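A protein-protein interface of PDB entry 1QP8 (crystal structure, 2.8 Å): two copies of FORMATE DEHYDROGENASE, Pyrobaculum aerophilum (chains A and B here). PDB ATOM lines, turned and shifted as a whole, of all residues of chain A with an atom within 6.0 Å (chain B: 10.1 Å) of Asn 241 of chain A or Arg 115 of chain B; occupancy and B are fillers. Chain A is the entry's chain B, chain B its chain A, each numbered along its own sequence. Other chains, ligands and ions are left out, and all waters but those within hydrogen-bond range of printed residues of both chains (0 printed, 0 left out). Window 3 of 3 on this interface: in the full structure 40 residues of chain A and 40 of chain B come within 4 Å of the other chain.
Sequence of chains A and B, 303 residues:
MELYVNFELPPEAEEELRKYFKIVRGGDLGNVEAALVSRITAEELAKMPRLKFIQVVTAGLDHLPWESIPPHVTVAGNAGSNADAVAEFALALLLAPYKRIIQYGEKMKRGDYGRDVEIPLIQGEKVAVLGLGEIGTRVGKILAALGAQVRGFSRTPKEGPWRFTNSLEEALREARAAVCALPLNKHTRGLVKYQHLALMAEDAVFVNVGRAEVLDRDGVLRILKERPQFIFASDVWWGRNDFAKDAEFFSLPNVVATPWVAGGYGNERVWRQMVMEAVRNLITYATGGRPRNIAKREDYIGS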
ATOM      1  N   ARG A  39     -18.810 -12.616  -2.717  1.00  0.00           N
ATOM      2  CA  ARG A  39     -17.521 -12.546  -2.044  1.00  0.00           C
ATOM      3  C   ARG A  39     -17.562 -11.273  -1.207  1.00  0.00           C
ATOM      4  O   ARG A  39     -18.479 -10.459  -1.357  1.00  0.00           O
ATOM      5  CB  ARG A  39     -16.371 -12.448  -3.050  1.00  0.00           C
ATOM      6  CG  ARG A  39     -16.087 -13.709  -3.849  1.00  0.00           C
ATOM      7  CD  ARG A  39     -14.911 -13.470  -4.790  1.00  0.00           C
ATOM      8  NE  ARG A  39     -14.575 -14.639  -5.596  1.00  0.00           N
ATOM      9  CZ  ARG A  39     -13.641 -14.643  -6.543  1.00  0.00           C
ATOM     10  NH1 ARG A  39     -12.953 -13.538  -6.798  1.00  0.00           N
ATOM     11  NH2 ARG A  39     -13.396 -15.747  -7.234  1.00  0.00           N
ATOM     12  N   TRP A 237     -10.667 -26.587  -9.004  1.00  0.00           N
ATOM     13  CA  TRP A 237      -9.216 -26.654  -8.925  1.00  0.00           C
ATOM     14  C   TRP A 237      -8.539 -25.780  -7.895  1.00  0.00           C
ATOM     15  O   TRP A 237      -9.098 -24.794  -7.428  1.00  0.00           O
ATOM     16  CB  TRP A 237      -8.625 -26.361 -10.306  1.00  0.00           C
ATOM     17  CG  TRP A 237      -9.229 -27.229 -11.331  1.00  0.00           C
ATOM     18  CD1 TRP A 237     -10.440 -27.052 -11.939  1.00  0.00           C
ATOM     19  CD2 TRP A 237      -8.750 -28.507 -11.750  1.00  0.00           C
ATOM     20  NE1 TRP A 237     -10.756 -28.154 -12.700  1.00  0.00           N
ATOM     21  CE2 TRP A 237      -9.732 -29.063 -12.606  1.00  0.00           C
ATOM     22  CE3 TRP A 237      -7.588 -29.242 -11.485  1.00  0.00           C
ATOM     23  CZ2 TRP A 237      -9.585 -30.326 -13.203  1.00  0.00           C
ATOM     24  CZ3 TRP A 237      -7.436 -30.501 -12.082  1.00  0.00           C
ATOM     25  CH2 TRP A 237      -8.435 -31.026 -12.932  1.00  0.00           C
ATOM     26  N   GLY A 239      -6.185 -23.861  -8.403  1.00  0.00           N
ATOM     27  CA  GLY A 239      -6.004 -22.547  -8.991  1.00  0.00           C
ATOM     28  C   GLY A 239      -7.217 -21.661  -8.782  1.00  0.00           C
ATOM     29  O   GLY A 239      -7.167 -20.467  -9.061  1.00  0.00           O
ATOM     30  N   ARG A 240      -8.303 -22.250  -8.292  1.00  0.00           N
ATOM     31  CA  ARG A 240      -9.549 -21.532  -8.027  1.00  0.00           C
ATOM     32  C   ARG A 240      -9.767 -20.373  -8.992  1.00  0.00           C
ATOM     33  O   ARG A 240      -9.467 -19.227  -8.669  1.00  0.00           O
ATOM     34  CB  ARG A 240      -9.565 -21.011  -6.576  1.00  0.00           C
ATOM     35  CG  ARG A 240     -10.974 -20.827  -5.968  1.00  0.00           C
ATOM     36  CD  ARG A 240     -11.316 -19.367  -5.618  1.00  0.00           C
ATOM     37  NE  ARG A 240     -12.691 -19.214  -5.125  1.00  0.00           N
ATOM     38  CZ  ARG A 240     -13.270 -18.050  -4.824  1.00  0.00           C
ATOM     39  NH1 ARG A 240     -12.598 -16.914  -4.959  1.00  0.00           N
ATOM     40  NH2 ARG A 240     -14.527 -18.018  -4.394  1.00  0.00           N
ATOM     41  N   ASN A 241     -10.285 -20.669 -10.177  1.00  0.00           N
ATOM     42  CA  ASN A 241     -10.560 -19.630 -11.180  1.00  0.00           C
ATOM     43  C   ASN A 241      -9.381 -19.203 -12.069  1.00  0.00           C
ATOM     44  O   ASN A 241      -9.589 -18.570 -13.111  1.00  0.00           O
ATOM     45  CB  ASN A 241     -11.160 -18.378 -10.518  1.00  0.00           C
ATOM     46  CG  ASN A 241     -12.673 -18.439 -10.414  1.00  0.00           C
ATOM     47  OD1 ASN A 241     -13.375 -18.446 -11.425  1.00  0.00           O
ATOM     48  ND2 ASN A 241     -13.182 -18.489  -9.188  1.00  0.00           N
ATOM     49  N   ASP A 242      -8.157 -19.525 -11.661  1.00  0.00           N
ATOM     50  CA  ASP A 242      -6.996 -19.181 -12.470  1.00  0.00           C
ATOM     51  C   ASP A 242      -6.879 -20.261 -13.538  1.00  0.00           C
ATOM     52  O   ASP A 242      -6.817 -19.970 -14.738  1.00  0.00           O
ATOM     53  CB  ASP A 242      -5.717 -19.173 -11.628  1.00  0.00           C
ATOM     54  CG  ASP A 242      -4.528 -18.580 -12.377  1.00  0.00           C
ATOM     55  OD1 ASP A 242      -4.427 -18.784 -13.604  1.00  0.00           O
ATOM     56  OD2 ASP A 242      -3.684 -17.917 -11.741  1.00  0.00           O
ATOM     57  N   PHE A 243      -6.847 -21.510 -13.080  1.00  0.00           N
ATOM     58  CA  PHE A 243      -6.751 -22.679 -13.955  1.00  0.00           C
ATOM     59  C   PHE A 243      -5.350 -22.847 -14.526  1.00  0.00           C
ATOM     60  O   PHE A 243      -4.704 -23.879 -14.329  1.00  0.00           O
ATOM     61  CB  PHE A 243      -7.766 -22.571 -15.098  1.00  0.00           C
ATOM     62  CG  PHE A 243      -9.203 -22.692 -14.656  1.00  0.00           C
ATOM     63  CD1 PHE A 243     -10.186 -21.916 -15.247  1.00  0.00           C
ATOM     64  CD2 PHE A 243      -9.578 -23.603 -13.672  1.00  0.00           C
ATOM     65  CE1 PHE A 243     -11.523 -22.046 -14.868  1.00  0.00           C
ATOM     66  CE2 PHE A 243     -10.918 -23.736 -13.289  1.00  0.00           C
ATOM     67  CZ  PHE A 243     -11.888 -22.958 -13.888  1.00  0.00           C
ATOM     68  N   PRO A 259     -14.037 -26.428 -16.199  1.00  0.00           N
ATOM     69  CA  PRO A 259     -13.865 -25.087 -15.622  1.00  0.00           C
ATOM     70  C   PRO A 259     -14.816 -24.633 -14.517  1.00  0.00           C
ATOM     71  O   PRO A 259     -15.353 -23.523 -14.598  1.00  0.00           O
ATOM     72  CB  PRO A 259     -13.979 -24.190 -16.838  1.00  0.00           C
ATOM     73  CG  PRO A 259     -15.077 -24.884 -17.616  1.00  0.00           C
ATOM     74  CD  PRO A 259     -14.678 -26.349 -17.527  1.00  0.00           C
ATOM     75  N   TRP A 260     -15.030 -25.465 -13.500  1.00  0.00           N
ATOM     76  CA  TRP A 260     -15.904 -25.081 -12.400  1.00  0.00           C
ATOM     77  C   TRP A 260     -17.258 -24.647 -12.960  1.00  0.00           C
ATOM     78  O   TRP A 260     -17.720 -23.542 -12.696  1.00  0.00           O
ATOM     79  CB  TRP A 260     -15.264 -23.920 -11.648  1.00  0.00           C
ATOM     80  CG  TRP A 260     -15.799 -23.663 -10.286  1.00  0.00           C
ATOM     81  CD1 TRP A 260     -17.040 -23.971  -9.810  1.00  0.00           C
ATOM     82  CD2 TRP A 260     -15.114 -22.998  -9.221  1.00  0.00           C
ATOM     83  NE1 TRP A 260     -17.170 -23.538  -8.514  1.00  0.00           N
ATOM     84  CE2 TRP A 260     -16.002 -22.936  -8.128  1.00  0.00           C
ATOM     85  CE3 TRP A 260     -13.833 -22.442  -9.087  1.00  0.00           C
ATOM     86  CZ2 TRP A 260     -15.648 -22.342  -6.911  1.00  0.00           C
ATOM     87  CZ3 TRP A 260     -13.483 -21.850  -7.877  1.00  0.00           C
ATOM     88  CH2 TRP A 260     -14.388 -21.805  -6.806  1.00  0.00           C
ATOM     89  N   VAL A 261     -17.896 -25.525 -13.728  1.00  0.00           N
ATOM     90  CA  VAL A 261     -19.179 -25.201 -14.332  1.00  0.00           C
ATOM     91  C   VAL A 261     -20.324 -26.124 -13.931  1.00  0.00           C
ATOM     92  O   VAL A 261     -21.390 -26.100 -14.553  1.00  0.00           O
ATOM     93  CB  VAL A 261     -19.045 -25.210 -15.861  1.00  0.00           C
ATOM     94  CG1 VAL A 261     -18.257 -23.995 -16.317  1.00  0.00           C
ATOM     95  CG2 VAL A 261     -18.328 -26.477 -16.303  1.00  0.00           C
ATOM     96  N   TYR A 265     -21.913 -21.224 -12.181  1.00  0.00           N
ATOM     97  CA  TYR A 265     -21.181 -20.486 -13.200  1.00  0.00           C
ATOM     98  C   TYR A 265     -21.341 -21.169 -14.557  1.00  0.00           C
ATOM     99  O   TYR A 265     -20.851 -20.669 -15.570  1.00  0.00           O
ATOM    100  CB  TYR A 265     -19.699 -20.417 -12.822  1.00  0.00           C
ATOM    101  CG  TYR A 265     -19.438 -19.685 -11.524  1.00  0.00           C
ATOM    102  CD1 TYR A 265     -18.213 -19.805 -10.864  1.00  0.00           C
ATOM    103  CD2 TYR A 265     -20.419 -18.875 -10.946  1.00  0.00           C
ATOM    104  CE1 TYR A 265     -17.971 -19.141  -9.659  1.00  0.00           C
ATOM    105  CE2 TYR A 265     -20.193 -18.206  -9.746  1.00  0.00           C
ATOM    106  CZ  TYR A 265     -18.968 -18.343  -9.106  1.00  0.00           C
ATOM    107  OH  TYR A 265     -18.754 -17.682  -7.914  1.00  0.00           O
ATOM    108  N   GLY A 266     -22.038 -22.304 -14.578  1.00  0.00           N
ATOM    109  CA  GLY A 266     -22.220 -23.031 -15.823  1.00  0.00           C
ATOM    110  C   GLY A 266     -23.616 -22.998 -16.408  1.00  0.00           C
ATOM    111  O   GLY A 266     -23.806 -23.342 -17.576  1.00  0.00           O
ATOM    112  N   ARG B 100     -21.879 -31.787 -21.333  1.00  0.00           N
ATOM    113  CA  ARG B 100     -20.730 -31.165 -21.987  1.00  0.00           C
ATOM    114  C   ARG B 100     -19.373 -31.530 -21.360  1.00  0.00           C
ATOM    115  O   ARG B 100     -18.419 -30.743 -21.416  1.00  0.00           O
ATOM    116  CB  ARG B 100     -20.917 -29.648 -21.955  1.00  0.00           C
ATOM    117  CG  ARG B 100     -22.371 -29.181 -22.170  1.00  0.00           C
ATOM    118  CD  ARG B 100     -22.719 -28.917 -23.630  1.00  0.00           C
ATOM    119  NE  ARG B 100     -23.761 -29.800 -24.145  1.00  0.00           N
ATOM    120  CZ  ARG B 100     -24.850 -29.374 -24.785  1.00  0.00           C
ATOM    121  NH1 ARG B 100     -25.049 -28.068 -24.982  1.00  0.00           N
ATOM    122  NH2 ARG B 100     -25.738 -30.245 -25.258  1.00  0.00           N
ATOM    123  N   TYR B 104     -15.939 -29.706 -22.762  1.00  0.00           N
ATOM    124  CA  TYR B 104     -15.134 -28.857 -21.889  1.00  0.00           C
ATOM    125  C   TYR B 104     -13.767 -29.472 -21.588  1.00  0.00           C
ATOM    126  O   TYR B 104     -12.777 -28.763 -21.431  1.00  0.00           O
ATOM    127  CB  TYR B 104     -15.882 -28.544 -20.586  1.00  0.00           C
ATOM    128  CG  TYR B 104     -16.657 -27.238 -20.634  1.00  0.00           C
ATOM    129  CD1 TYR B 104     -18.053 -27.222 -20.608  1.00  0.00           C
ATOM    130  CD2 TYR B 104     -15.992 -26.018 -20.715  1.00  0.00           C
ATOM    131  CE1 TYR B 104     -18.776 -26.019 -20.664  1.00  0.00           C
ATOM    132  CE2 TYR B 104     -16.705 -24.804 -20.768  1.00  0.00           C
ATOM    133  CZ  TYR B 104     -18.099 -24.814 -20.744  1.00  0.00           C
ATOM    134  OH  TYR B 104     -18.796 -23.627 -20.809  1.00  0.00           O
ATOM    135  N   LYS B 107     -11.599 -28.344 -24.331  1.00  0.00           N
ATOM    136  CA  LYS B 107     -11.236 -26.940 -24.201  1.00  0.00           C
ATOM    137  C   LYS B 107     -10.181 -26.739 -23.125  1.00  0.00           C
ATOM    138  O   LYS B 107      -9.272 -25.936 -23.299  1.00  0.00           O
ATOM    139  CB  LYS B 107     -12.475 -26.105 -23.912  1.00  0.00           C
ATOM    140  CG  LYS B 107     -13.577 -26.346 -24.955  1.00  0.00           C
ATOM    141  CD  LYS B 107     -14.827 -25.517 -24.693  1.00  0.00           C
ATOM    142  CE  LYS B 107     -14.486 -24.044 -24.688  1.00  0.00           C
ATOM    143  NZ  LYS B 107     -15.687 -23.205 -24.789  1.00  0.00           N
ATOM    144  N   MET B 108     -10.279 -27.485 -22.027  1.00  0.00           N
ATOM    145  CA  MET B 108      -9.296 -27.355 -20.958  1.00  0.00           C
ATOM    146  C   MET B 108      -7.927 -27.787 -21.478  1.00  0.00           C
ATOM    147  O   MET B 108      -6.917 -27.103 -21.267  1.00  0.00           O
ATOM    148  CB  MET B 108      -9.680 -28.224 -19.757  1.00  0.00           C
ATOM    149  CG  MET B 108     -10.855 -27.717 -18.928  1.00  0.00           C
ATOM    150  SD  MET B 108     -10.540 -26.184 -18.007  1.00  0.00           S
ATOM    151  CE  MET B 108     -11.595 -25.059 -18.940  1.00  0.00           C
ATOM    152  N   GLY B 111      -6.080 -25.297 -23.548  1.00  0.00           N
ATOM    153  CA  GLY B 111      -5.773 -24.032 -22.903  1.00  0.00           C
ATOM    154  C   GLY B 111      -6.943 -23.085 -22.791  1.00  0.00           C
ATOM    155  O   GLY B 111      -6.860 -22.067 -22.106  1.00  0.00           O
ATOM    156  N   ASP B 112      -8.034 -23.410 -23.470  1.00  0.00           N
ATOM    157  CA  ASP B 112      -9.227 -22.575 -23.431  1.00  0.00           C
ATOM    158  C   ASP B 112      -9.927 -22.779 -22.074  1.00  0.00           C
ATOM    159  O   ASP B 112     -10.397 -23.875 -21.760  1.00  0.00           O
ATOM    160  CB  ASP B 112     -10.144 -22.970 -24.588  1.00  0.00           C
ATOM    161  CG  ASP B 112     -11.370 -22.100 -24.686  1.00  0.00           C
ATOM    162  OD1 ASP B 112     -11.596 -21.280 -23.767  1.00  0.00           O
ATOM    163  OD2 ASP B 112     -12.114 -22.245 -25.687  1.00  0.00           O
ATOM    164  N   TYR B 113      -9.987 -21.729 -21.263  1.00  0.00           N
ATOM    165  CA  TYR B 113     -10.618 -21.833 -19.946  1.00  0.00           C
ATOM    166  C   TYR B 113     -11.901 -21.013 -19.850  1.00  0.00           C
ATOM    167  O   TYR B 113     -12.350 -20.674 -18.762  1.00  0.00           O
ATOM    168  CB  TYR B 113      -9.640 -21.376 -18.855  1.00  0.00           C
ATOM    169  CG  TYR B 113      -8.299 -22.072 -18.895  1.00  0.00           C
ATOM    170  CD1 TYR B 113      -7.138 -21.401 -18.504  1.00  0.00           C
ATOM    171  CD2 TYR B 113      -8.181 -23.400 -19.325  1.00  0.00           C
ATOM    172  CE1 TYR B 113      -5.885 -22.028 -18.542  1.00  0.00           C
ATOM    173  CE2 TYR B 113      -6.933 -24.041 -19.365  1.00  0.00           C
ATOM    174  CZ  TYR B 113      -5.793 -23.346 -18.972  1.00  0.00           C
ATOM    175  OH  TYR B 113      -4.556 -23.945 -19.017  1.00  0.00           O
ATOM    176  N   GLY B 114     -12.490 -20.697 -20.992  1.00  0.00           N
ATOM    177  CA  GLY B 114     -13.712 -19.925 -20.975  1.00  0.00           C
ATOM    178  C   GLY B 114     -14.889 -20.792 -20.591  1.00  0.00           C
ATOM    179  O   GLY B 114     -14.834 -22.018 -20.719  1.00  0.00           O
ATOM    180  N   ARG B 115     -15.947 -20.149 -20.110  1.00  0.00           N
ATOM    181  CA  ARG B 115     -17.164 -20.836 -19.713  1.00  0.00           C
ATOM    182  C   ARG B 115     -18.249 -20.342 -20.650  1.00  0.00           C
ATOM    183  O   ARG B 115     -19.327 -19.941 -20.219  1.00  0.00           O
ATOM    184  CB  ARG B 115     -17.536 -20.496 -18.263  1.00  0.00           C
ATOM    185  CG  ARG B 115     -16.440 -20.795 -17.248  1.00  0.00           C
ATOM    186  CD  ARG B 115     -16.960 -20.724 -15.814  1.00  0.00           C
ATOM    187  NE  ARG B 115     -16.173 -19.788 -15.018  1.00  0.00           N
ATOM    188  CZ  ARG B 115     -15.904 -19.929 -13.725  1.00  0.00           C
ATOM    189  NH1 ARG B 115     -16.362 -20.976 -13.056  1.00  0.00           N
ATOM    190  NH2 ARG B 115     -15.149 -19.032 -13.103  1.00  0.00           N
ATOM    191  N   ASP B 116     -17.950 -20.373 -21.942  1.00  0.00           N
ATOM    192  CA  ASP B 116     -18.889 -19.910 -22.957  1.00  0.00           C
ATOM    193  C   ASP B 116     -19.991 -20.883 -23.318  1.00  0.00           C
ATOM    194  O   ASP B 116     -20.947 -20.498 -23.978  1.00  0.00           O
ATOM    195  CB  ASP B 116     -18.141 -19.575 -24.237  1.00  0.00           C
ATOM    196  CG  ASP B 116     -17.273 -20.721 -24.702  1.00  0.00           C
ATOM    197  OD1 ASP B 116     -16.175 -20.903 -24.115  1.00  0.00           O
ATOM    198  OD2 ASP B 116     -17.700 -21.438 -25.636  1.00  0.00           O
ATOM    199  N   VAL B 117     -19.853 -22.142 -22.922  1.00  0.00           N
ATOM    200  CA  VAL B 117     -20.868 -23.151 -23.247  1.00  0.00           C
ATOM    201  C   VAL B 117     -21.774 -23.386 -22.048  1.00  0.00           C
ATOM    202  O   VAL B 117     -21.289 -23.694 -20.956  1.00  0.00           O
ATOM    203  CB  VAL B 117     -20.236 -24.527 -23.586  1.00  0.00           C
ATOM    204  CG1 VAL B 117     -21.315 -25.493 -24.036  1.00  0.00           C
ATOM    205  CG2 VAL B 117     -19.174 -24.379 -24.646  1.00  0.00           C
ATOM    206  N   GLU B 118     -23.083 -23.250 -22.229  1.00  0.00           N
ATOM    207  CA  GLU B 118     -23.974 -23.487 -21.100  1.00  0.00           C
ATOM    208  C   GLU B 118     -24.220 -24.982 -20.919  1.00  0.00           C
ATOM    209  O   GLU B 118     -24.355 -25.737 -21.890  1.00  0.00           O
ATOM    210  CB  GLU B 118     -25.305 -22.748 -21.263  1.00  0.00           C
ATOM    211  CG  GLU B 118     -26.215 -22.905 -20.045  1.00  0.00           C
ATOM    212  CD  GLU B 118     -27.255 -21.805 -19.917  1.00  0.00           C
ATOM    213  OE1 GLU B 118     -28.057 -21.613 -20.858  1.00  0.00           O
ATOM    214  OE2 GLU B 118     -27.273 -21.134 -18.863  1.00  0.00           O
ATOM    215  N   ILE B 119     -24.261 -25.401 -19.661  1.00  0.00           N
ATOM    216  CA  ILE B 119     -24.471 -26.794 -19.313  1.00  0.00           C
ATOM    217  C   ILE B 119     -25.948 -27.114 -19.144  1.00  0.00           C
ATOM    218  O   ILE B 119     -26.610 -26.588 -18.260  1.00  0.00           O
ATOM    219  CB  ILE B 119     -23.680 -27.107 -18.051  1.00  0.00           C
ATOM    220  CG1 ILE B 119     -22.200 -26.890 -18.373  1.00  0.00           C
ATOM    221  CG2 ILE B 119     -23.957 -28.523 -17.580  1.00  0.00           C
ATOM    222  CD1 ILE B 119     -21.266 -27.191 -17.265  1.00  0.00           C
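Hydrophobic or aromatic side chains of chain A within 4 Å of the printed part of chain B: Phe 243, Pro 259, Trp 260, Val 261 and Tyr 265. Printed residues of chain B that touch a printed residue of chain A: Tyr 104, Met 108, Tyr 113, Arg 115, Glu 118 and Ile 119. Along chain B the printed residues that touch a printed residue of chain A span positions 104 to 119. Among the printed residues, 11 pairs touch across the chains. Among the printed residues, no Asp or Glu carboxylate lies within 4 Å of a Lys or Arg side-chain nitrogen of the other chain.
Among the printed residues, pairs that only touch across the chains: Val 261 of chain A with Ile 119 of chain B, Tyr 265 of chain A with Arg 115 of chain B, Pro 259 of chain A with Met 108 of chain B, Pro 259 of chain A with Tyr 104 of chain B, Gly 266 of chain A with Glu 118 of chain B, Val 261 of chain A with Arg 115 of chain B and Phe 243 of chain A with Tyr 113 of chain B.
No position is printed for both chains. Of the 11 pairs that touch across the chains among the printed residues, none has its exchanged pair printed and touching as well.
OH of Tyr 104 of chain B sits at hydrogen-bond distance from O of Val 117 of chain B (2.5 Å). The guanidinium group of Arg 39 of chain A sits close to the side-chain amide nitrogen of Asn 241 of chain A.
Asn 241 of chain A touches one residue of chain B. Of the printed residues of chain B, Phe 243 of chain A touches Tyr 113. Of the printed residues of chain B, Pro 259 of chain A touches Tyr 104 (3.4 Å), Met 108 (3.3 Å) and Arg 115 (3.1 Å). Trp 260 of chain A touches one residue of chain B. Tyr 265 of chain A touches just one residue of chain B: Arg 115. Arg 115 of chain B touches just these residues of chain A: Asn 241, Pro 259, Trp 260, Val 261 and Tyr 265. Printed residues of chain A within 4 Å of Ile 119 of chain B: Val 261 and Gly 266. The nearest residue of chain A that does not touch Arg 115 of chain B is Phe 243 of chain A (5.0 Å). The nearest printed residue of chain B that does not touch Pro 259 of chain A is Gly 114 of chain B (4.2 Å).
The guanidinium group of Arg 115 of chain B lies within hydrogen-bond range of the side-chain amide oxygen of Asn 241 of chain A (2.5 Å). NH1 of Arg 115 of chain B is in hydrogen-bond range of O of Pro 259 of chain A, 3.1 Å away. The backbone carbonyl oxygen (O) of Trp 260 of chain A sits at hydrogen-bond distance from the guanidinium group (NH1) of Arg 115 of chain B. The backbone NH (N) of Ile 119 of chain B sits at hydrogen-bond distance from the backbone carbonyl oxygen (O) of Gly 266 of chain A (3.0 Å).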
